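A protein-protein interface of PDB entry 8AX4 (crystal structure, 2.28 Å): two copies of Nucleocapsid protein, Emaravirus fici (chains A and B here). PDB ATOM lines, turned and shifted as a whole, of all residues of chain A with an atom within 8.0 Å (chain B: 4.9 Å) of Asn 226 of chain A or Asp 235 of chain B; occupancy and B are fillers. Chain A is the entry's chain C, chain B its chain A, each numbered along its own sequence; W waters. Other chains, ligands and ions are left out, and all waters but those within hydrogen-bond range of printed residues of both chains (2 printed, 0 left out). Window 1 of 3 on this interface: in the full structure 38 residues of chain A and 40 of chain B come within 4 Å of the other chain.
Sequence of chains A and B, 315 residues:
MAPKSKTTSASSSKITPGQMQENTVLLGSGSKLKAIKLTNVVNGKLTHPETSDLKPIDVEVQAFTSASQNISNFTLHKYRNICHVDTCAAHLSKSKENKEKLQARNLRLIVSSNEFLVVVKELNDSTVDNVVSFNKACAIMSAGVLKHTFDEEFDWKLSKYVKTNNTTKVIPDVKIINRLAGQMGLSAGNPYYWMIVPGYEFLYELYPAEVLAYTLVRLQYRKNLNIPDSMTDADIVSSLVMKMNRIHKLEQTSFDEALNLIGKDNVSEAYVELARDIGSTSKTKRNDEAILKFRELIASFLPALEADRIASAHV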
ATOM      1  N   GLN A 183      20.358   2.542   9.361  1.00  0.00           N
ATOM      2  CA  GLN A 183      21.505   1.747   8.937  1.00  0.00           C
ATOM      3  C   GLN A 183      22.234   2.399   7.769  1.00  0.00           C
ATOM      4  O   GLN A 183      23.445   2.210   7.612  1.00  0.00           O
ATOM      5  CB  GLN A 183      21.057   0.334   8.567  1.00  0.00           C
ATOM      6  CG  GLN A 183      22.162  -0.703   8.656  1.00  0.00           C
ATOM      7  CD  GLN A 183      22.071  -1.744   7.559  1.00  0.00           C
ATOM      8  OE1 GLN A 183      21.038  -1.887   6.907  1.00  0.00           O
ATOM      9  NE2 GLN A 183      23.157  -2.477   7.350  1.00  0.00           N
ATOM     10  N   TYR A 221      26.862  -0.034  -2.222  1.00  0.00           N
ATOM     11  CA  TYR A 221      27.285  -0.203  -0.833  1.00  0.00           C
ATOM     12  C   TYR A 221      26.760  -1.491  -0.211  1.00  0.00           C
ATOM     13  O   TYR A 221      26.349  -1.491   0.953  1.00  0.00           O
ATOM     14  CB  TYR A 221      26.852   1.007  -0.012  1.00  0.00           C
ATOM     15  CG  TYR A 221      27.507   2.292  -0.463  1.00  0.00           C
ATOM     16  CD1 TYR A 221      28.873   2.485  -0.314  1.00  0.00           C
ATOM     17  CD2 TYR A 221      26.763   3.307  -1.051  1.00  0.00           C
ATOM     18  CE1 TYR A 221      29.481   3.655  -0.727  1.00  0.00           C
ATOM     19  CE2 TYR A 221      27.361   4.482  -1.470  1.00  0.00           C
ATOM     20  CZ  TYR A 221      28.722   4.651  -1.305  1.00  0.00           C
ATOM     21  OH  TYR A 221      29.327   5.815  -1.718  1.00  0.00           O
ATOM     22  N   ARG A 222      26.773  -2.592  -0.972  1.00  0.00           N
ATOM     23  CA  ARG A 222      26.376  -3.905  -0.470  1.00  0.00           C
ATOM     24  C   ARG A 222      26.906  -4.172   0.932  1.00  0.00           C
ATOM     25  O   ARG A 222      26.151  -4.513   1.850  1.00  0.00           O
ATOM     26  CB  ARG A 222      26.893  -5.000  -1.406  1.00  0.00           C
ATOM     27  CG  ARG A 222      26.518  -4.882  -2.858  1.00  0.00           C
ATOM     28  CD  ARG A 222      27.053  -6.106  -3.572  1.00  0.00           C
ATOM     29  NE  ARG A 222      26.705  -7.319  -2.838  1.00  0.00           N
ATOM     30  CZ  ARG A 222      25.920  -8.281  -3.307  1.00  0.00           C
ATOM     31  NH1 ARG A 222      25.408  -8.186  -4.526  1.00  0.00           N
ATOM     32  NH2 ARG A 222      25.653  -9.345  -2.559  1.00  0.00           N
ATOM     33  N   LYS A 223      28.220  -4.020   1.099  1.00  0.00           N
ATOM     34  CA  LYS A 223      28.869  -4.395   2.351  1.00  0.00           C
ATOM     35  C   LYS A 223      28.388  -3.521   3.500  1.00  0.00           C
ATOM     36  O   LYS A 223      28.086  -4.018   4.592  1.00  0.00           O
ATOM     37  CB  LYS A 223      30.387  -4.299   2.196  1.00  0.00           C
ATOM     38  CG  LYS A 223      30.948  -5.057   0.996  1.00  0.00           C
ATOM     39  CD  LYS A 223      30.269  -6.409   0.813  1.00  0.00           C
ATOM     40  CE  LYS A 223      30.511  -6.970  -0.578  1.00  0.00           C
ATOM     41  NZ  LYS A 223      31.844  -7.623  -0.689  1.00  0.00           N
ATOM     42  N   ASN A 224      28.302  -2.208   3.267  1.00  0.00           N
ATOM     43  CA  ASN A 224      27.875  -1.292   4.319  1.00  0.00           C
ATOM     44  C   ASN A 224      26.451  -1.574   4.769  1.00  0.00           C
ATOM     45  O   ASN A 224      26.104  -1.321   5.927  1.00  0.00           O
ATOM     46  CB  ASN A 224      27.993   0.153   3.836  1.00  0.00           C
ATOM     47  CG  ASN A 224      29.403   0.516   3.425  1.00  0.00           C
ATOM     48  OD1 ASN A 224      29.832   0.218   2.310  1.00  0.00           O
ATOM     49  ND2 ASN A 224      30.133   1.164   4.324  1.00  0.00           N
ATOM     50  N   LEU A 225      25.614  -2.096   3.875  1.00  0.00           N
ATOM     51  CA  LEU A 225      24.203  -2.307   4.162  1.00  0.00           C
ATOM     52  C   LEU A 225      23.897  -3.753   4.536  1.00  0.00           C
ATOM     53  O   LEU A 225      22.725  -4.144   4.552  1.00  0.00           O
ATOM     54  CB  LEU A 225      23.351  -1.860   2.969  1.00  0.00           C
ATOM     55  CG  LEU A 225      23.017  -0.365   2.821  1.00  0.00           C
ATOM     56  CD1 LEU A 225      24.153   0.561   3.254  1.00  0.00           C
ATOM     57  CD2 LEU A 225      22.605  -0.049   1.390  1.00  0.00           C
ATOM     58  N   ASN A 226      24.929  -4.549   4.833  1.00  0.00           N
ATOM     59  CA  ASN A 226      24.774  -5.903   5.374  1.00  0.00           C
ATOM     60  C   ASN A 226      23.994  -6.808   4.422  1.00  0.00           C
ATOM     61  O   ASN A 226      23.232  -7.677   4.847  1.00  0.00           O
ATOM     62  CB  ASN A 226      24.119  -5.868   6.757  1.00  0.00           C
ATOM     63  CG  ASN A 226      24.322  -7.155   7.533  1.00  0.00           C
ATOM     64  OD1 ASN A 226      25.356  -7.812   7.413  1.00  0.00           O
ATOM     65  ND2 ASN A 226      23.329  -7.523   8.334  1.00  0.00           N
ATOM     66  N   ILE A 227      24.190  -6.608   3.128  1.00  0.00           N
ATOM     67  CA  ILE A 227      23.475  -7.402   2.125  1.00  0.00           C
ATOM     68  C   ILE A 227      24.197  -8.736   1.947  1.00  0.00           C
ATOM     69  O   ILE A 227      25.424  -8.745   1.757  1.00  0.00           O
ATOM     70  CB  ILE A 227      23.383  -6.642   0.807  1.00  0.00           C
ATOM     71  CG1 ILE A 227      22.578  -5.353   1.002  1.00  0.00           C
ATOM     72  CG2 ILE A 227      22.744  -7.510  -0.266  1.00  0.00           C
ATOM     73  CD1 ILE A 227      22.243  -4.635  -0.286  1.00  0.00           C
ATOM     74  N   PRO A 228      23.490  -9.861   2.009  1.00  0.00           N
ATOM     75  CA  PRO A 228      24.162 -11.163   1.926  1.00  0.00           C
ATOM     76  C   PRO A 228      24.785 -11.405   0.561  1.00  0.00           C
ATOM     77  O   PRO A 228      24.334 -10.881  -0.460  1.00  0.00           O
ATOM     78  CB  PRO A 228      23.033 -12.164   2.201  1.00  0.00           C
ATOM     79  CG  PRO A 228      21.772 -11.418   1.886  1.00  0.00           C
ATOM     80  CD  PRO A 228      22.045  -9.995   2.258  1.00  0.00           C
ATOM     81  N   ASP A 229      25.844 -12.220   0.560  1.00  0.00           N
ATOM     82  CA  ASP A 229      26.450 -12.656  -0.693  1.00  0.00           C
ATOM     83  C   ASP A 229      25.508 -13.529  -1.508  1.00  0.00           C
ATOM     84  O   ASP A 229      25.671 -13.630  -2.729  1.00  0.00           O
ATOM     85  CB  ASP A 229      27.750 -13.417  -0.422  1.00  0.00           C
ATOM     86  CG  ASP A 229      28.816 -12.548   0.217  1.00  0.00           C
ATOM     87  OD1 ASP A 229      28.679 -11.308   0.179  1.00  0.00           O
ATOM     88  OD2 ASP A 229      29.794 -13.110   0.753  1.00  0.00           O
ATOM     89  N   MET A 231      22.719 -12.807  -2.384  1.00  0.00           N
ATOM     90  CA  MET A 231      21.975 -11.907  -3.254  1.00  0.00           C
ATOM     91  C   MET A 231      22.913 -11.418  -4.351  1.00  0.00           C
ATOM     92  O   MET A 231      23.837 -10.642  -4.086  1.00  0.00           O
ATOM     93  CB  MET A 231      21.403 -10.735  -2.461  1.00  0.00           C
ATOM     94  CG  MET A 231      19.941 -10.889  -2.088  1.00  0.00           C
ATOM     95  SD  MET A 231      19.233  -9.336  -1.512  1.00  0.00           S
ATOM     96  CE  MET A 231      18.928  -8.514  -3.071  1.00  0.00           C
ATOM     97  N   THR A 284      29.518  -2.557  13.800  1.00  0.00           N
ATOM     98  CA  THR A 284      29.816  -3.293  12.573  1.00  0.00           C
ATOM     99  C   THR A 284      31.306  -3.577  12.433  1.00  0.00           C
ATOM    100  O   THR A 284      31.696  -4.604  11.867  1.00  0.00           O
ATOM    101  CB  THR A 284      29.292  -2.532  11.353  1.00  0.00           C
ATOM    102  OG1 THR A 284      30.117  -1.384  11.115  1.00  0.00           O
ATOM    103  CG2 THR A 284      27.853  -2.093  11.546  1.00  0.00           C
ATOM    104  N   ASN A 287      31.911  -6.640  14.721  1.00  0.00           N
ATOM    105  CA  ASN A 287      31.549  -7.880  14.041  1.00  0.00           C
ATOM    106  C   ASN A 287      32.595  -8.264  13.002  1.00  0.00           C
ATOM    107  O   ASN A 287      32.984  -9.433  12.906  1.00  0.00           O
ATOM    108  CB  ASN A 287      30.173  -7.739  13.389  1.00  0.00           C
ATOM    109  CG  ASN A 287      29.049  -7.690  14.405  1.00  0.00           C
ATOM    110  OD1 ASN A 287      29.234  -8.042  15.571  1.00  0.00           O
ATOM    111  ND2 ASN A 287      27.872  -7.255  13.967  1.00  0.00           N
ATOM    112  N   ASP A 288      33.073  -7.289  12.225  1.00  0.00           N
ATOM    113  CA  ASP A 288      34.049  -7.584  11.181  1.00  0.00           C
ATOM    114  C   ASP A 288      35.379  -8.035  11.775  1.00  0.00           C
ATOM    115  O   ASP A 288      36.014  -8.960  11.255  1.00  0.00           O
ATOM    116  CB  ASP A 288      34.242  -6.364  10.283  1.00  0.00           C
ATOM    117  CG  ASP A 288      33.046  -6.107   9.388  1.00  0.00           C
ATOM    118  OD1 ASP A 288      32.203  -7.018   9.242  1.00  0.00           O
ATOM    119  OD2 ASP A 288      32.948  -4.994   8.829  1.00  0.00           O
ATOM    120  N   ILE A 291      34.887 -11.605  13.033  1.00  0.00           N
ATOM    121  CA  ILE A 291      34.920 -12.612  11.976  1.00  0.00           C
ATOM    122  C   ILE A 291      36.358 -12.961  11.616  1.00  0.00           C
ATOM    123  O   ILE A 291      36.689 -14.131  11.396  1.00  0.00           O
ATOM    124  CB  ILE A 291      34.125 -12.130  10.749  1.00  0.00           C
ATOM    125  CG1 ILE A 291      32.651 -11.946  11.111  1.00  0.00           C
ATOM    126  CG2 ILE A 291      34.257 -13.116   9.605  1.00  0.00           C
ATOM    127  CD1 ILE A 291      31.884 -11.095  10.125  1.00  0.00           C
ATOM    128  N   SER B 230      20.155 -16.018   3.496  1.00  0.00           N
ATOM    129  CA  SER B 230      19.789 -14.623   3.703  1.00  0.00           C
ATOM    130  C   SER B 230      20.628 -13.955   4.784  1.00  0.00           C
ATOM    131  O   SER B 230      20.542 -12.733   4.944  1.00  0.00           O
ATOM    132  CB  SER B 230      18.309 -14.514   4.072  1.00  0.00           C
ATOM    133  OG  SER B 230      18.106 -14.785   5.450  1.00  0.00           O
ATOM    134  N   MET B 231      21.430 -14.721   5.518  1.00  0.00           N
ATOM    135  CA  MET B 231      22.181 -14.222   6.660  1.00  0.00           C
ATOM    136  C   MET B 231      23.641 -14.017   6.280  1.00  0.00           C
ATOM    137  O   MET B 231      24.264 -14.903   5.686  1.00  0.00           O
ATOM    138  CB  MET B 231      22.085 -15.201   7.831  1.00  0.00           C
ATOM    139  CG  MET B 231      20.873 -15.006   8.718  1.00  0.00           C
ATOM    140  SD  MET B 231      20.883 -16.165  10.097  1.00  0.00           S
ATOM    141  CE  MET B 231      21.848 -15.252  11.296  1.00  0.00           C
ATOM    142  N   THR B 232      24.181 -12.855   6.631  1.00  0.00           N
ATOM    143  CA  THR B 232      25.601 -12.613   6.451  1.00  0.00           C
ATOM    144  C   THR B 232      26.397 -13.318   7.545  1.00  0.00           C
ATOM    145  O   THR B 232      25.854 -13.750   8.565  1.00  0.00           O
ATOM    146  CB  THR B 232      25.904 -11.113   6.474  1.00  0.00           C
ATOM    147  OG1 THR B 232      25.565 -10.574   7.759  1.00  0.00           O
ATOM    148  CG2 THR B 232      25.105 -10.394   5.402  1.00  0.00           C
ATOM    149  N   ASP B 233      27.706 -13.442   7.314  1.00  0.00           N
ATOM    150  CA  ASP B 233      28.584 -13.975   8.350  1.00  0.00           C
ATOM    151  C   ASP B 233      28.508 -13.130   9.615  1.00  0.00           C
ATOM    152  O   ASP B 233      28.609 -13.654  10.731  1.00  0.00           O
ATOM    153  CB  ASP B 233      30.023 -14.045   7.838  1.00  0.00           C
ATOM    154  CG  ASP B 233      30.228 -15.146   6.815  1.00  0.00           C
ATOM    155  OD1 ASP B 233      29.370 -16.049   6.725  1.00  0.00           O
ATOM    156  OD2 ASP B 233      31.253 -15.108   6.102  1.00  0.00           O
ATOM    157  N   ALA B 234      28.322 -11.816   9.459  1.00  0.00           N
ATOM    158  CA  ALA B 234      28.179 -10.941  10.618  1.00  0.00           C
ATOM    159  C   ALA B 234      26.857 -11.174  11.337  1.00  0.00           C
ATOM    160  O   ALA B 234      26.785 -11.016  12.561  1.00  0.00           O
ATOM    161  CB  ALA B 234      28.305  -9.479  10.192  1.00  0.00           C
ATOM    162  N   ASP B 235      25.802 -11.534  10.598  1.00  0.00           N
ATOM    163  CA  ASP B 235      24.549 -11.927  11.234  1.00  0.00           C
ATOM    164  C   ASP B 235      24.753 -13.105  12.174  1.00  0.00           C
ATOM    165  O   ASP B 235      24.068 -13.214  13.198  1.00  0.00           O
ATOM    166  CB  ASP B 235      23.505 -12.292  10.175  1.00  0.00           C
ATOM    167  CG  ASP B 235      22.914 -11.081   9.482  1.00  0.00           C
ATOM    168  OD1 ASP B 235      22.981  -9.972  10.051  1.00  0.00           O
ATOM    169  OD2 ASP B 235      22.376 -11.246   8.365  1.00  0.00           O
ATOM    170  N   ILE B 236      25.697 -13.989  11.844  1.00  0.00           N
ATOM    171  CA  ILE B 236      25.896 -15.212  12.612  1.00  0.00           C
ATOM    172  C   ILE B 236      26.579 -14.922  13.942  1.00  0.00           C
ATOM    173  O   ILE B 236      26.308 -15.594  14.947  1.00  0.00           O
ATOM    174  CB  ILE B 236      26.692 -16.219  11.758  1.00  0.00           C
ATOM    175  CG1 ILE B 236      25.839 -16.696  10.579  1.00  0.00           C
ATOM    176  CG2 ILE B 236      27.168 -17.396  12.592  1.00  0.00           C
ATOM    177  CD1 ILE B 236      26.516 -17.732   9.710  1.00  0.00           C
ATOM    178  N   VAL B 237      27.449 -13.914  13.988  1.00  0.00           N
ATOM    179  CA  VAL B 237      28.257 -13.646  15.173  1.00  0.00           C
ATOM    180  C   VAL B 237      27.789 -12.433  15.961  1.00  0.00           C
ATOM    181  O   VAL B 237      28.280 -12.223  17.083  1.00  0.00           O
ATOM    182  CB  VAL B 237      29.748 -13.482  14.807  1.00  0.00           C
ATOM    183  CG1 VAL B 237      30.186 -14.585  13.858  1.00  0.00           C
ATOM    184  CG2 VAL B 237      29.994 -12.112  14.193  1.00  0.00           C
ATOM    185  N   SER B 238      26.853 -11.640  15.434  1.00  0.00           N
ATOM    186  CA  SER B 238      26.532 -10.354  16.050  1.00  0.00           C
ATOM    187  C   SER B 238      26.026 -10.517  17.479  1.00  0.00           C
ATOM    188  O   SER B 238      26.429  -9.762  18.375  1.00  0.00           O
ATOM    189  CB  SER B 238      25.501  -9.608  15.204  1.00  0.00           C
ATOM    190  OG  SER B 238      25.189  -8.352  15.782  1.00  0.00           O
HETATM  191  O   HOH W   1      27.538  -6.975  17.547  1.00  0.00           O
HETATM  192  O   HOH W   2      21.714  -9.434   6.580  1.00  0.00           O
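The side-chain hydroxyl of Thr 232 of chain B is in hydrogen-bond range of the side-chain amide oxygen of Asn 226 of chain A (2.8 Å).
ND2 of Asn 287 of chain A is in hydrogen-bond range of OG of Ser 238 of chain B.
The side-chain amide nitrogen of Asn 226 of chain A sits at hydrogen-bond distance from the side-chain carboxylate of Asp 235 of chain B, at 3.0 Å.
O of Pro 228 of chain A lies within hydrogen-bond range of NH2 of Arg 222 of chain A (2.9 Å).
OG1 of Thr 232 of chain B sits close to N of Ala 234 of chain B.
N of Ile 227 of chain A sits at hydrogen-bond distance from O of Arg 222 of chain A.
The backbone NH (N) of Thr 232 of chain B is in hydrogen-bond range of the side-chain carboxylate (OD2) of Asp 235 of chain B.
Among the printed residues, pairs that only touch across the chains: Pro 228 of chain A with Ser 230 of chain B, Pro 228 of chain A with Thr 232 of chain B, Ile 291 of chain A with Ala 234 of chain B, Ile 227 of chain A with Thr 232 of chain B and Ile 291 of chain A with Asp 233 of chain B.
Of chain B, only Thr 232 and Asp 235 come within 4 Å of Asn 226 of chain A.
Printed residues of chain B within 4 Å of Pro 228 of chain A: Ser 230 and Thr 232.
Met 231 of chain A touches none of the printed residues of chain B.
Of the printed residues of chain B, Asn 287 of chain A touches Ser 238.
Of the printed residues of chain A, Ser 230 of chain B touches Pro 228 (3.5 Å).
Ala 234 of chain B touches just one residue of chain A: Ile 291 (3.7 Å).
Of chain A, only Asn 226 comes within 4 Å of Asp 235 of chain B.
Of the printed residues of chain A, Ser 238 of chain B touches Asn 287 (3.4 Å).
The nearest residue of chain B that does not touch Asn 226 of chain A is Ala 234 of chain B (4.4 Å).
The nearest residue of chain A that does not touch Asp 235 of chain B is Asn 287 of chain A (5.8 Å).
The nearest printed residue of chain A that does not touch Ser 238 of chain B is Ile 291 of chain A (7.2 Å).
Of the 15 printed residues of chain A, 5 touch a printed residue of chain B.
Printed residues of chain A that touch a printed residue of chain B: Asn 226, Ile 227, Pro 228, Asn 287 and Ile 291.
Hydrophobic or aromatic side chains of chain A that line the printed part of chain B: Pro 228 and Ile 291.
Of the 9 printed residues of chain B, 6 touch a printed residue of chain A.
Among the printed residues, no Asp or Glu carboxylate lies within 4 Å of a Lys or Arg side-chain nitrogen of the other chain.
Position printed for both chains: 231.
Of the 8 pairs that touch across the chains among the printed residues, none has its exchanged pair printed and touching as well.
Water W2 bridges the side-chain carboxylate of Asp 235 of chain B (2.6 Å) and the backbone carbonyl oxygen of Asn 226 of chain A (2.9 Å).
Water W1 lies within hydrogen-bond range of the side-chain amide oxygen (OD1) of Asn 287 of chain A (2.8 Å) and the backbone carbonyl oxygen (O) of Ser 238 of chain B (3.1 Å).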
